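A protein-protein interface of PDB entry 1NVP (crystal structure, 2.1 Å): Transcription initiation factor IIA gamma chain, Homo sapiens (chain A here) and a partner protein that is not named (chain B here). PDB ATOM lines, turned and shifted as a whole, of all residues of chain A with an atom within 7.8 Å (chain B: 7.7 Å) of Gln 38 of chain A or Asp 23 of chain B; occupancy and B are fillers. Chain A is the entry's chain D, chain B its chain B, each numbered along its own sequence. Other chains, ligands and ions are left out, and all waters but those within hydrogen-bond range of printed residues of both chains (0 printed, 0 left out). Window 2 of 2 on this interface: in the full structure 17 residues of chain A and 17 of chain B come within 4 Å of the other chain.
Printed residues of chain B within 4 Å of Leu 14 of chain A: Trp 45 (3.7 Å). Of chain B, only Asp 23 and Val 24 come within 4 Å of Gln 38 of chain A. Lys 41 of chain A touches none of the printed residues of chain B. Of the printed residues of chain B, Ala 42 of chain A touches Val 20. Of the printed residues of chain A, Val 20 of chain B touches Ala 42 (3.7 Å). Of chain A, only Gln 38 (3.4 Å) comes within 4 Å of Asp 23 of chain B. Of the printed residues of chain A, Ile 27 of chain B touches Leu 31 (3.4 Å). Printed residues of chain A within 4 Å of Phe 28 of chain B: Leu 31 (3.9 Å) and Val 35 (3.9 Å). The nearest residue of chain B that does not touch Gln 38 of chain A is Val 20 of chain B (4.3 Å). The nearest residue of chain A that does not touch Asp 23 of chain B is Ala 42 of chain A (6.1 Å). The nearest printed residue of chain B that does not touch Leu 14 of chain A is Val 20 of chain B (5.3 Å).
Among the printed residues, merely in contact across the chains: Leu 14 of chain A with Trp 45 of chain B (3.7 Å), Leu 31 of chain A with Ile 27 of chain B (3.4 Å), Leu 31 of chain A with Phe 28 of chain B (3.9 Å), Val 35 of chain A with Phe 28 of chain B (3.9 Å), Gln 38 of chain A with Asp 23 of chain B (3.4 Å), Gln 38 of chain A with Val 24 of chain B (3.8 Å) and Ala 42 of chain A with Val 20 of chain B (3.7 Å).
Of the 16 printed residues of chain A, 5 touch a printed residue of chain B. Hydrophobic or aromatic side chains of chain A that line the printed part of chain B: Leu 14, Leu 31, Val 35 and Ala 42. Printed residues of chain B that touch a printed residue of chain A: Val 20, Asp 23, Val 24, Ile 27, Phe 28 and Trp 45. Hydrophobic or aromatic side chains of chain B within 4 Å of the printed part of chain A: Val 20, Val 24, Ile 27, Phe 28 and Trp 45. Among the printed residues, 7 pairs touch across the chains.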
ATOM      1  N   ARG A   6      -0.177  12.652  19.426  1.00  0.00           N
ATOM      2  CA  ARG A   6      -0.337  11.209  19.475  1.00  0.00           C
ATOM      3  C   ARG A   6       0.929  10.482  19.925  1.00  0.00           C
ATOM      4  O   ARG A   6       0.840   9.450  20.593  1.00  0.00           O
ATOM      5  CB  ARG A   6      -0.806  10.678  18.122  1.00  0.00           C
ATOM      6  CG  ARG A   6      -2.184  11.191  17.746  1.00  0.00           C
ATOM      7  CD  ARG A   6      -2.820  10.363  16.651  1.00  0.00           C
ATOM      8  NE  ARG A   6      -4.086  10.945  16.215  1.00  0.00           N
ATOM      9  CZ  ARG A   6      -4.868  10.408  15.286  1.00  0.00           C
ATOM     10  NH1 ARG A   6      -4.517   9.276  14.696  1.00  0.00           N
ATOM     11  NH2 ARG A   6      -5.998  11.008  14.939  1.00  0.00           N
ATOM     12  N   LEU A  14      -2.380   5.017  24.518  1.00  0.00           N
ATOM     13  CA  LEU A  14      -3.694   4.857  23.906  1.00  0.00           C
ATOM     14  C   LEU A  14      -3.636   3.972  22.661  1.00  0.00           C
ATOM     15  O   LEU A  14      -4.396   3.010  22.532  1.00  0.00           O
ATOM     16  CB  LEU A  14      -4.272   6.231  23.544  1.00  0.00           C
ATOM     17  CG  LEU A  14      -5.591   6.275  22.761  1.00  0.00           C
ATOM     18  CD1 LEU A  14      -6.670   5.480  23.492  1.00  0.00           C
ATOM     19  CD2 LEU A  14      -6.019   7.722  22.586  1.00  0.00           C
ATOM     20  N   LEU A  31     -12.763   1.898  14.130  1.00  0.00           N
ATOM     21  CA  LEU A  31     -13.196   2.358  15.442  1.00  0.00           C
ATOM     22  C   LEU A  31     -12.011   2.950  16.190  1.00  0.00           C
ATOM     23  O   LEU A  31     -12.142   3.970  16.871  1.00  0.00           O
ATOM     24  CB  LEU A  31     -13.800   1.199  16.252  1.00  0.00           C
ATOM     25  CG  LEU A  31     -14.366   1.592  17.623  1.00  0.00           C
ATOM     26  CD1 LEU A  31     -15.441   2.661  17.445  1.00  0.00           C
ATOM     27  CD2 LEU A  31     -14.942   0.363  18.319  1.00  0.00           C
ATOM     28  N   ALA A  32     -10.857   2.298  16.066  1.00  0.00           N
ATOM     29  CA  ALA A  32      -9.633   2.762  16.716  1.00  0.00           C
ATOM     30  C   ALA A  32      -9.292   4.158  16.195  1.00  0.00           C
ATOM     31  O   ALA A  32      -8.956   5.059  16.968  1.00  0.00           O
ATOM     32  CB  ALA A  32      -8.485   1.796  16.430  1.00  0.00           C
ATOM     33  N   LEU A  33      -9.385   4.326  14.879  1.00  0.00           N
ATOM     34  CA  LEU A  33      -9.109   5.616  14.258  1.00  0.00           C
ATOM     35  C   LEU A  33     -10.053   6.668  14.827  1.00  0.00           C
ATOM     36  O   LEU A  33      -9.642   7.790  15.138  1.00  0.00           O
ATOM     37  CB  LEU A  33      -9.300   5.540  12.742  1.00  0.00           C
ATOM     38  CG  LEU A  33      -9.125   6.890  12.032  1.00  0.00           C
ATOM     39  CD1 LEU A  33      -7.705   7.397  12.258  1.00  0.00           C
ATOM     40  CD2 LEU A  33      -9.419   6.751  10.544  1.00  0.00           C
ATOM     41  N   GLN A  34     -11.322   6.295  14.963  1.00  0.00           N
ATOM     42  CA  GLN A  34     -12.326   7.201  15.497  1.00  0.00           C
ATOM     43  C   GLN A  34     -11.994   7.612  16.925  1.00  0.00           C
ATOM     44  O   GLN A  34     -12.266   8.741  17.332  1.00  0.00           O
ATOM     45  CB  GLN A  34     -13.704   6.543  15.450  1.00  0.00           C
ATOM     46  CG  GLN A  34     -14.246   6.319  14.046  1.00  0.00           C
ATOM     47  CD  GLN A  34     -14.520   7.619  13.312  1.00  0.00           C
ATOM     48  OE1 GLN A  34     -14.525   8.696  13.913  1.00  0.00           O
ATOM     49  NE2 GLN A  34     -14.765   7.524  12.010  1.00  0.00           N
ATOM     50  N   VAL A  35     -11.407   6.695  17.689  1.00  0.00           N
ATOM     51  CA  VAL A  35     -11.035   6.988  19.069  1.00  0.00           C
ATOM     52  C   VAL A  35      -9.871   7.979  19.101  1.00  0.00           C
ATOM     53  O   VAL A  35      -9.850   8.911  19.912  1.00  0.00           O
ATOM     54  CB  VAL A  35     -10.594   5.717  19.815  1.00  0.00           C
ATOM     55  CG1 VAL A  35     -10.220   6.067  21.247  1.00  0.00           C
ATOM     56  CG2 VAL A  35     -11.700   4.677  19.771  1.00  0.00           C
ATOM     57  N   LEU A  36      -8.895   7.756  18.226  1.00  0.00           N
ATOM     58  CA  LEU A  36      -7.731   8.631  18.141  1.00  0.00           C
ATOM     59  C   LEU A  36      -8.194  10.028  17.759  1.00  0.00           C
ATOM     60  O   LEU A  36      -7.726  11.022  18.315  1.00  0.00           O
ATOM     61  CB  LEU A  36      -6.738   8.086  17.110  1.00  0.00           C
ATOM     62  CG  LEU A  36      -6.002   6.823  17.571  1.00  0.00           C
ATOM     63  CD1 LEU A  36      -5.289   6.169  16.400  1.00  0.00           C
ATOM     64  CD2 LEU A  36      -5.022   7.184  18.682  1.00  0.00           C
ATOM     65  N   LEU A  37      -9.132  10.102  16.820  1.00  0.00           N
ATOM     66  CA  LEU A  37      -9.656  11.397  16.408  1.00  0.00           C
ATOM     67  C   LEU A  37     -10.241  12.109  17.622  1.00  0.00           C
ATOM     68  O   LEU A  37     -10.026  13.306  17.815  1.00  0.00           O
ATOM     69  CB  LEU A  37     -10.725  11.224  15.326  1.00  0.00           C
ATOM     70  CG  LEU A  37     -10.176  10.809  13.958  1.00  0.00           C
ATOM     71  CD1 LEU A  37     -11.306  10.682  12.948  1.00  0.00           C
ATOM     72  CD2 LEU A  37      -9.161  11.848  13.494  1.00  0.00           C
ATOM     73  N   GLN A  38     -10.969  11.365  18.451  1.00  0.00           N
ATOM     74  CA  GLN A  38     -11.565  11.945  19.647  1.00  0.00           C
ATOM     75  C   GLN A  38     -10.465  12.419  20.585  1.00  0.00           C
ATOM     76  O   GLN A  38     -10.597  13.452  21.247  1.00  0.00           O
ATOM     77  CB  GLN A  38     -12.441  10.915  20.368  1.00  0.00           C
ATOM     78  CG  GLN A  38     -13.311  11.517  21.455  1.00  0.00           C
ATOM     79  CD  GLN A  38     -14.190  12.638  20.925  1.00  0.00           C
ATOM     80  OE1 GLN A  38     -14.870  12.478  19.910  1.00  0.00           O
ATOM     81  NE2 GLN A  38     -14.180  13.776  21.610  1.00  0.00           N
ATOM     82  N   PHE A  39      -9.379  11.655  20.644  1.00  0.00           N
ATOM     83  CA  PHE A  39      -8.252  12.001  21.499  1.00  0.00           C
ATOM     84  C   PHE A  39      -7.627  13.333  21.075  1.00  0.00           C
ATOM     85  O   PHE A  39      -7.325  14.181  21.921  1.00  0.00           O
ATOM     86  CB  PHE A  39      -7.189  10.896  21.452  1.00  0.00           C
ATOM     87  CG  PHE A  39      -5.873  11.298  22.056  1.00  0.00           C
ATOM     88  CD1 PHE A  39      -5.712  11.371  23.436  1.00  0.00           C
ATOM     89  CD2 PHE A  39      -4.799  11.636  21.236  1.00  0.00           C
ATOM     90  CE1 PHE A  39      -4.497  11.774  23.993  1.00  0.00           C
ATOM     91  CE2 PHE A  39      -3.581  12.039  21.782  1.00  0.00           C
ATOM     92  CZ  PHE A  39      -3.429  12.111  23.162  1.00  0.00           C
ATOM     93  N   ASP A  40      -7.434  13.514  19.769  1.00  0.00           N
ATOM     94  CA  ASP A  40      -6.839  14.752  19.260  1.00  0.00           C
ATOM     95  C   ASP A  40      -7.610  15.965  19.767  1.00  0.00           C
ATOM     96  O   ASP A  40      -7.026  16.888  20.335  1.00  0.00           O
ATOM     97  CB  ASP A  40      -6.813  14.772  17.724  1.00  0.00           C
ATOM     98  CG  ASP A  40      -5.935  13.680  17.130  1.00  0.00           C
ATOM     99  OD1 ASP A  40      -4.913  13.319  17.751  1.00  0.00           O
ATOM    100  OD2 ASP A  40      -6.259  13.189  16.028  1.00  0.00           O
ATOM    101  N   LYS A  41      -8.925  15.957  19.569  1.00  0.00           N
ATOM    102  CA  LYS A  41      -9.762  17.065  20.015  1.00  0.00           C
ATOM    103  C   LYS A  41      -9.631  17.283  21.519  1.00  0.00           C
ATOM    104  O   LYS A  41      -9.518  18.418  21.987  1.00  0.00           O
ATOM    105  CB  LYS A  41     -11.234  16.798  19.677  1.00  0.00           C
ATOM    106  CG  LYS A  41     -11.508  16.518  18.205  1.00  0.00           C
ATOM    107  CD  LYS A  41     -13.005  16.509  17.920  1.00  0.00           C
ATOM    108  CE  LYS A  41     -13.295  16.214  16.455  1.00  0.00           C
ATOM    109  NZ  LYS A  41     -14.728  16.458  16.108  1.00  0.00           N
ATOM    110  N   ALA A  42      -9.634  16.185  22.268  1.00  0.00           N
ATOM    111  CA  ALA A  42      -9.552  16.236  23.725  1.00  0.00           C
ATOM    112  C   ALA A  42      -8.227  16.735  24.302  1.00  0.00           C
ATOM    113  O   ALA A  42      -8.225  17.516  25.258  1.00  0.00           O
ATOM    114  CB  ALA A  42      -9.886  14.860  24.307  1.00  0.00           C
ATOM    115  N   ILE A  43      -7.104  16.288  23.746  1.00  0.00           N
ATOM    116  CA  ILE A  43      -5.808  16.729  24.259  1.00  0.00           C
ATOM    117  C   ILE A  43      -5.555  18.190  23.896  1.00  0.00           C
ATOM    118  O   ILE A  43      -5.058  18.965  24.716  1.00  0.00           O
ATOM    119  CB  ILE A  43      -4.643  15.852  23.725  1.00  0.00           C
ATOM    120  CG1 ILE A  43      -3.335  16.275  24.396  1.00  0.00           C
ATOM    121  CG2 ILE A  43      -4.524  15.981  22.215  1.00  0.00           C
ATOM    122  CD1 ILE A  43      -3.348  16.155  25.907  1.00  0.00           C
ATOM    123  N   ASN A  44      -5.911  18.564  22.670  1.00  0.00           N
ATOM    124  CA  ASN A  44      -5.738  19.936  22.209  1.00  0.00           C
ATOM    125  C   ASN A  44      -6.541  20.880  23.098  1.00  0.00           C
ATOM    126  O   ASN A  44      -6.022  21.883  23.585  1.00  0.00           O
ATOM    127  CB  ASN A  44      -6.204  20.072  20.754  1.00  0.00           C
ATOM    128  CG  ASN A  44      -5.143  19.639  19.750  1.00  0.00           C
ATOM    129  OD1 ASN A  44      -4.163  20.353  19.517  1.00  0.00           O
ATOM    130  ND2 ASN A  44      -5.331  18.464  19.152  1.00  0.00           N
ATOM    131  N   VAL B  16      -8.474  13.958  30.473  1.00  0.00           N
ATOM    132  CA  VAL B  16      -8.550  13.582  29.066  1.00  0.00           C
ATOM    133  C   VAL B  16      -9.075  12.167  28.857  1.00  0.00           C
ATOM    134  O   VAL B  16      -9.880  11.925  27.958  1.00  0.00           O
ATOM    135  CB  VAL B  16      -7.174  13.707  28.375  1.00  0.00           C
ATOM    136  CG1 VAL B  16      -7.261  13.193  26.945  1.00  0.00           C
ATOM    137  CG2 VAL B  16      -6.723  15.159  28.383  1.00  0.00           C
ATOM    138  N   ILE B  17      -8.611  11.226  29.672  1.00  0.00           N
ATOM    139  CA  ILE B  17      -9.070   9.848  29.548  1.00  0.00           C
ATOM    140  C   ILE B  17     -10.584   9.795  29.765  1.00  0.00           C
ATOM    141  O   ILE B  17     -11.309   9.159  28.998  1.00  0.00           O
ATOM    142  CB  ILE B  17      -8.355   8.921  30.566  1.00  0.00           C
ATOM    143  CG1 ILE B  17      -6.870   8.801  30.201  1.00  0.00           C
ATOM    144  CG2 ILE B  17      -9.010   7.542  30.575  1.00  0.00           C
ATOM    145  CD1 ILE B  17      -6.070   7.869  31.095  1.00  0.00           C
ATOM    146  N   GLU B  18     -11.058  10.484  30.799  1.00  0.00           N
ATOM    147  CA  GLU B  18     -12.486  10.514  31.096  1.00  0.00           C
ATOM    148  C   GLU B  18     -13.261  11.056  29.908  1.00  0.00           C
ATOM    149  O   GLU B  18     -14.186  10.409  29.414  1.00  0.00           O
ATOM    150  CB  GLU B  18     -12.768  11.383  32.326  1.00  0.00           C
ATOM    151  CG  GLU B  18     -12.204  10.837  33.633  1.00  0.00           C
ATOM    152  CD  GLU B  18     -12.668   9.419  33.935  1.00  0.00           C
ATOM    153  OE1 GLU B  18     -13.545   8.901  33.208  1.00  0.00           O
ATOM    154  OE2 GLU B  18     -12.157   8.823  34.907  1.00  0.00           O
ATOM    155  N   ASP B  19     -12.875  12.243  29.450  1.00  0.00           N
ATOM    156  CA  ASP B  19     -13.540  12.871  28.316  1.00  0.00           C
ATOM    157  C   ASP B  19     -13.544  11.976  27.084  1.00  0.00           C
ATOM    158  O   ASP B  19     -14.581  11.803  26.444  1.00  0.00           O
ATOM    159  CB  ASP B  19     -12.878  14.213  27.979  1.00  0.00           C
ATOM    160  CG  ASP B  19     -13.050  15.242  29.083  1.00  0.00           C
ATOM    161  OD1 ASP B  19     -13.862  14.994  30.000  1.00  0.00           O
ATOM    162  OD2 ASP B  19     -12.383  16.297  29.032  1.00  0.00           O
ATOM    163  N   VAL B  20     -12.392  11.403  26.749  1.00  0.00           N
ATOM    164  CA  VAL B  20     -12.315  10.537  25.577  1.00  0.00           C
ATOM    165  C   VAL B  20     -13.208   9.309  25.731  1.00  0.00           C
ATOM    166  O   VAL B  20     -13.957   8.958  24.820  1.00  0.00           O
ATOM    167  CB  VAL B  20     -10.867  10.058  25.306  1.00  0.00           C
ATOM    168  CG1 VAL B  20     -10.854   9.112  24.106  1.00  0.00           C
ATOM    169  CG2 VAL B  20      -9.955  11.259  25.047  1.00  0.00           C
ATOM    170  N   ILE B  21     -13.118   8.649  26.883  1.00  0.00           N
ATOM    171  CA  ILE B  21     -13.930   7.460  27.127  1.00  0.00           C
ATOM    172  C   ILE B  21     -15.411   7.816  27.018  1.00  0.00           C
ATOM    173  O   ILE B  21     -16.169   7.139  26.324  1.00  0.00           O
ATOM    174  CB  ILE B  21     -13.633   6.853  28.515  1.00  0.00           C
ATOM    175  CG1 ILE B  21     -12.178   6.377  28.565  1.00  0.00           C
ATOM    176  CG2 ILE B  21     -14.573   5.681  28.789  1.00  0.00           C
ATOM    177  CD1 ILE B  21     -11.824   5.353  27.490  1.00  0.00           C
ATOM    178  N   ASN B  22     -15.818   8.888  27.687  1.00  0.00           N
ATOM    179  CA  ASN B  22     -17.210   9.310  27.617  1.00  0.00           C
ATOM    180  C   ASN B  22     -17.611   9.636  26.184  1.00  0.00           C
ATOM    181  O   ASN B  22     -18.687   9.251  25.730  1.00  0.00           O
ATOM    182  CB  ASN B  22     -17.459  10.540  28.497  1.00  0.00           C
ATOM    183  CG  ASN B  22     -17.500  10.203  29.973  1.00  0.00           C
ATOM    184  OD1 ASN B  22     -17.953   9.125  30.362  1.00  0.00           O
ATOM    185  ND2 ASN B  22     -17.047  11.132  30.807  1.00  0.00           N
ATOM    186  N   ASP B  23     -16.739  10.329  25.458  1.00  0.00           N
ATOM    187  CA  ASP B  23     -17.054  10.717  24.087  1.00  0.00           C
ATOM    188  C   ASP B  23     -17.052   9.629  23.020  1.00  0.00           C
ATOM    189  O   ASP B  23     -17.537   9.865  21.913  1.00  0.00           O
ATOM    190  CB  ASP B  23     -16.148  11.870  23.647  1.00  0.00           C
ATOM    191  CG  ASP B  23     -16.622  13.210  24.177  1.00  0.00           C
ATOM    192  OD1 ASP B  23     -17.762  13.603  23.856  1.00  0.00           O
ATOM    193  OD2 ASP B  23     -15.861  13.870  24.912  1.00  0.00           O
ATOM    194  N   VAL B  24     -16.527   8.445  23.323  1.00  0.00           N
ATOM    195  CA  VAL B  24     -16.523   7.372  22.326  1.00  0.00           C
ATOM    196  C   VAL B  24     -17.554   6.276  22.624  1.00  0.00           C
ATOM    197  O   VAL B  24     -17.796   5.388  21.801  1.00  0.00           O
ATOM    198  CB  VAL B  24     -15.123   6.711  22.195  1.00  0.00           C
ATOM    199  CG1 VAL B  24     -14.080   7.768  21.810  1.00  0.00           C
ATOM    200  CG2 VAL B  24     -14.742   6.023  23.498  1.00  0.00           C
ATOM    201  N   ARG B  25     -18.158   6.349  23.805  1.00  0.00           N
ATOM    202  CA  ARG B  25     -19.164   5.374  24.216  1.00  0.00           C
ATOM    203  C   ARG B  25     -20.210   5.162  23.118  1.00  0.00           C
ATOM    204  O   ARG B  25     -20.430   4.031  22.673  1.00  0.00           O
ATOM    205  CB  ARG B  25     -19.823   5.842  25.523  1.00  0.00           C
ATOM    206  CG  ARG B  25     -20.812   4.856  26.139  1.00  0.00           C
ATOM    207  CD  ARG B  25     -21.020   5.146  27.621  1.00  0.00           C
ATOM    208  NE  ARG B  25     -20.002   4.510  28.453  1.00  0.00           N
ATOM    209  CZ  ARG B  25     -19.159   5.157  29.254  1.00  0.00           C
ATOM    210  NH1 ARG B  25     -19.201   6.480  29.340  1.00  0.00           N
ATOM    211  NH2 ARG B  25     -18.278   4.477  29.979  1.00  0.00           N
ATOM    212  N   ASP B  26     -20.834   6.244  22.653  1.00  0.00           N
ATOM    213  CA  ASP B  26     -21.844   6.123  21.606  1.00  0.00           C
ATOM    214  C   ASP B  26     -21.306   5.491  20.336  1.00  0.00           C
ATOM    215  O   ASP B  26     -22.016   4.740  19.662  1.00  0.00           O
ATOM    216  CB  ASP B  26     -22.454   7.486  21.264  1.00  0.00           C
ATOM    217  CG  ASP B  26     -23.283   8.054  22.398  1.00  0.00           C
ATOM    218  OD1 ASP B  26     -23.764   7.264  23.237  1.00  0.00           O
ATOM    219  OD2 ASP B  26     -23.461   9.290  22.443  1.00  0.00           O
ATOM    220  N   ILE B  27     -20.053   5.789  20.001  1.00  0.00           N
ATOM    221  CA  ILE B  27     -19.460   5.228  18.789  1.00  0.00           C
ATOM    222  C   ILE B  27     -19.327   3.720  18.938  1.00  0.00           C
ATOM    223  O   ILE B  27     -19.604   2.967  18.006  1.00  0.00           O
ATOM    224  CB  ILE B  27     -18.068   5.825  18.500  1.00  0.00           C
ATOM    225  CG1 ILE B  27     -18.153   7.354  18.471  1.00  0.00           C
ATOM    226  CG2 ILE B  27     -17.553   5.304  17.161  1.00  0.00           C
ATOM    227  CD1 ILE B  27     -16.839   8.040  18.144  1.00  0.00           C
ATOM    228  N   PHE B  28     -18.886   3.283  20.115  1.00  0.00           N
ATOM    229  CA  PHE B  28     -18.748   1.855  20.381  1.00  0.00           C
ATOM    230  C   PHE B  28     -20.127   1.212  20.262  1.00  0.00           C
ATOM    231  O   PHE B  28     -20.291   0.170  19.620  1.00  0.00           O
ATOM    232  CB  PHE B  28     -18.196   1.617  21.789  1.00  0.00           C
ATOM    233  CG  PHE B  28     -16.695   1.584  21.860  1.00  0.00           C
ATOM    234  CD1 PHE B  28     -16.042   0.499  22.446  1.00  0.00           C
ATOM    235  CD2 PHE B  28     -15.930   2.635  21.356  1.00  0.00           C
ATOM    236  CE1 PHE B  28     -14.648   0.461  22.536  1.00  0.00           C
ATOM    237  CE2 PHE B  28     -14.535   2.607  21.440  1.00  0.00           C
ATOM    238  CZ  PHE B  28     -13.894   1.516  22.031  1.00  0.00           C
ATOM    239  N   LEU B  38     -15.211  -1.162  25.978  1.00  0.00           N
ATOM    240  CA  LEU B  38     -14.867   0.223  26.246  1.00  0.00           C
ATOM    241  C   LEU B  38     -14.106   0.312  27.562  1.00  0.00           C
ATOM    242  O   LEU B  38     -13.062   0.968  27.648  1.00  0.00           O
ATOM    243  CB  LEU B  38     -16.123   1.094  26.323  1.00  0.00           C
ATOM    244  CG  LEU B  38     -15.855   2.585  26.586  1.00  0.00           C
ATOM    245  CD1 LEU B  38     -15.075   3.175  25.418  1.00  0.00           C
ATOM    246  CD2 LEU B  38     -17.169   3.332  26.774  1.00  0.00           C
ATOM    247  N   TRP B  45      -5.440   1.423  28.887  1.00  0.00           N
ATOM    248  CA  TRP B  45      -4.881   2.759  28.756  1.00  0.00           C
ATOM    249  C   TRP B  45      -4.332   3.334  30.061  1.00  0.00           C
ATOM    250  O   TRP B  45      -3.184   3.783  30.109  1.00  0.00           O
ATOM    251  CB  TRP B  45      -5.949   3.694  28.182  1.00  0.00           C
ATOM    252  CG  TRP B  45      -5.439   5.043  27.765  1.00  0.00           C
ATOM    253  CD1 TRP B  45      -4.136   5.469  27.750  1.00  0.00           C
ATOM    254  CD2 TRP B  45      -6.224   6.140  27.284  1.00  0.00           C
ATOM    255  NE1 TRP B  45      -4.065   6.763  27.288  1.00  0.00           N
ATOM    256  CE2 TRP B  45      -5.331   7.200  26.995  1.00  0.00           C
ATOM    257  CE3 TRP B  45      -7.596   6.332  27.068  1.00  0.00           C
ATOM    258  CZ2 TRP B  45      -5.766   8.435  26.500  1.00  0.00           C
ATOM    259  CZ3 TRP B  45      -8.032   7.562  26.576  1.00  0.00           C
ATOM    260  CH2 TRP B  45      -7.116   8.597  26.297  1.00  0.00           C
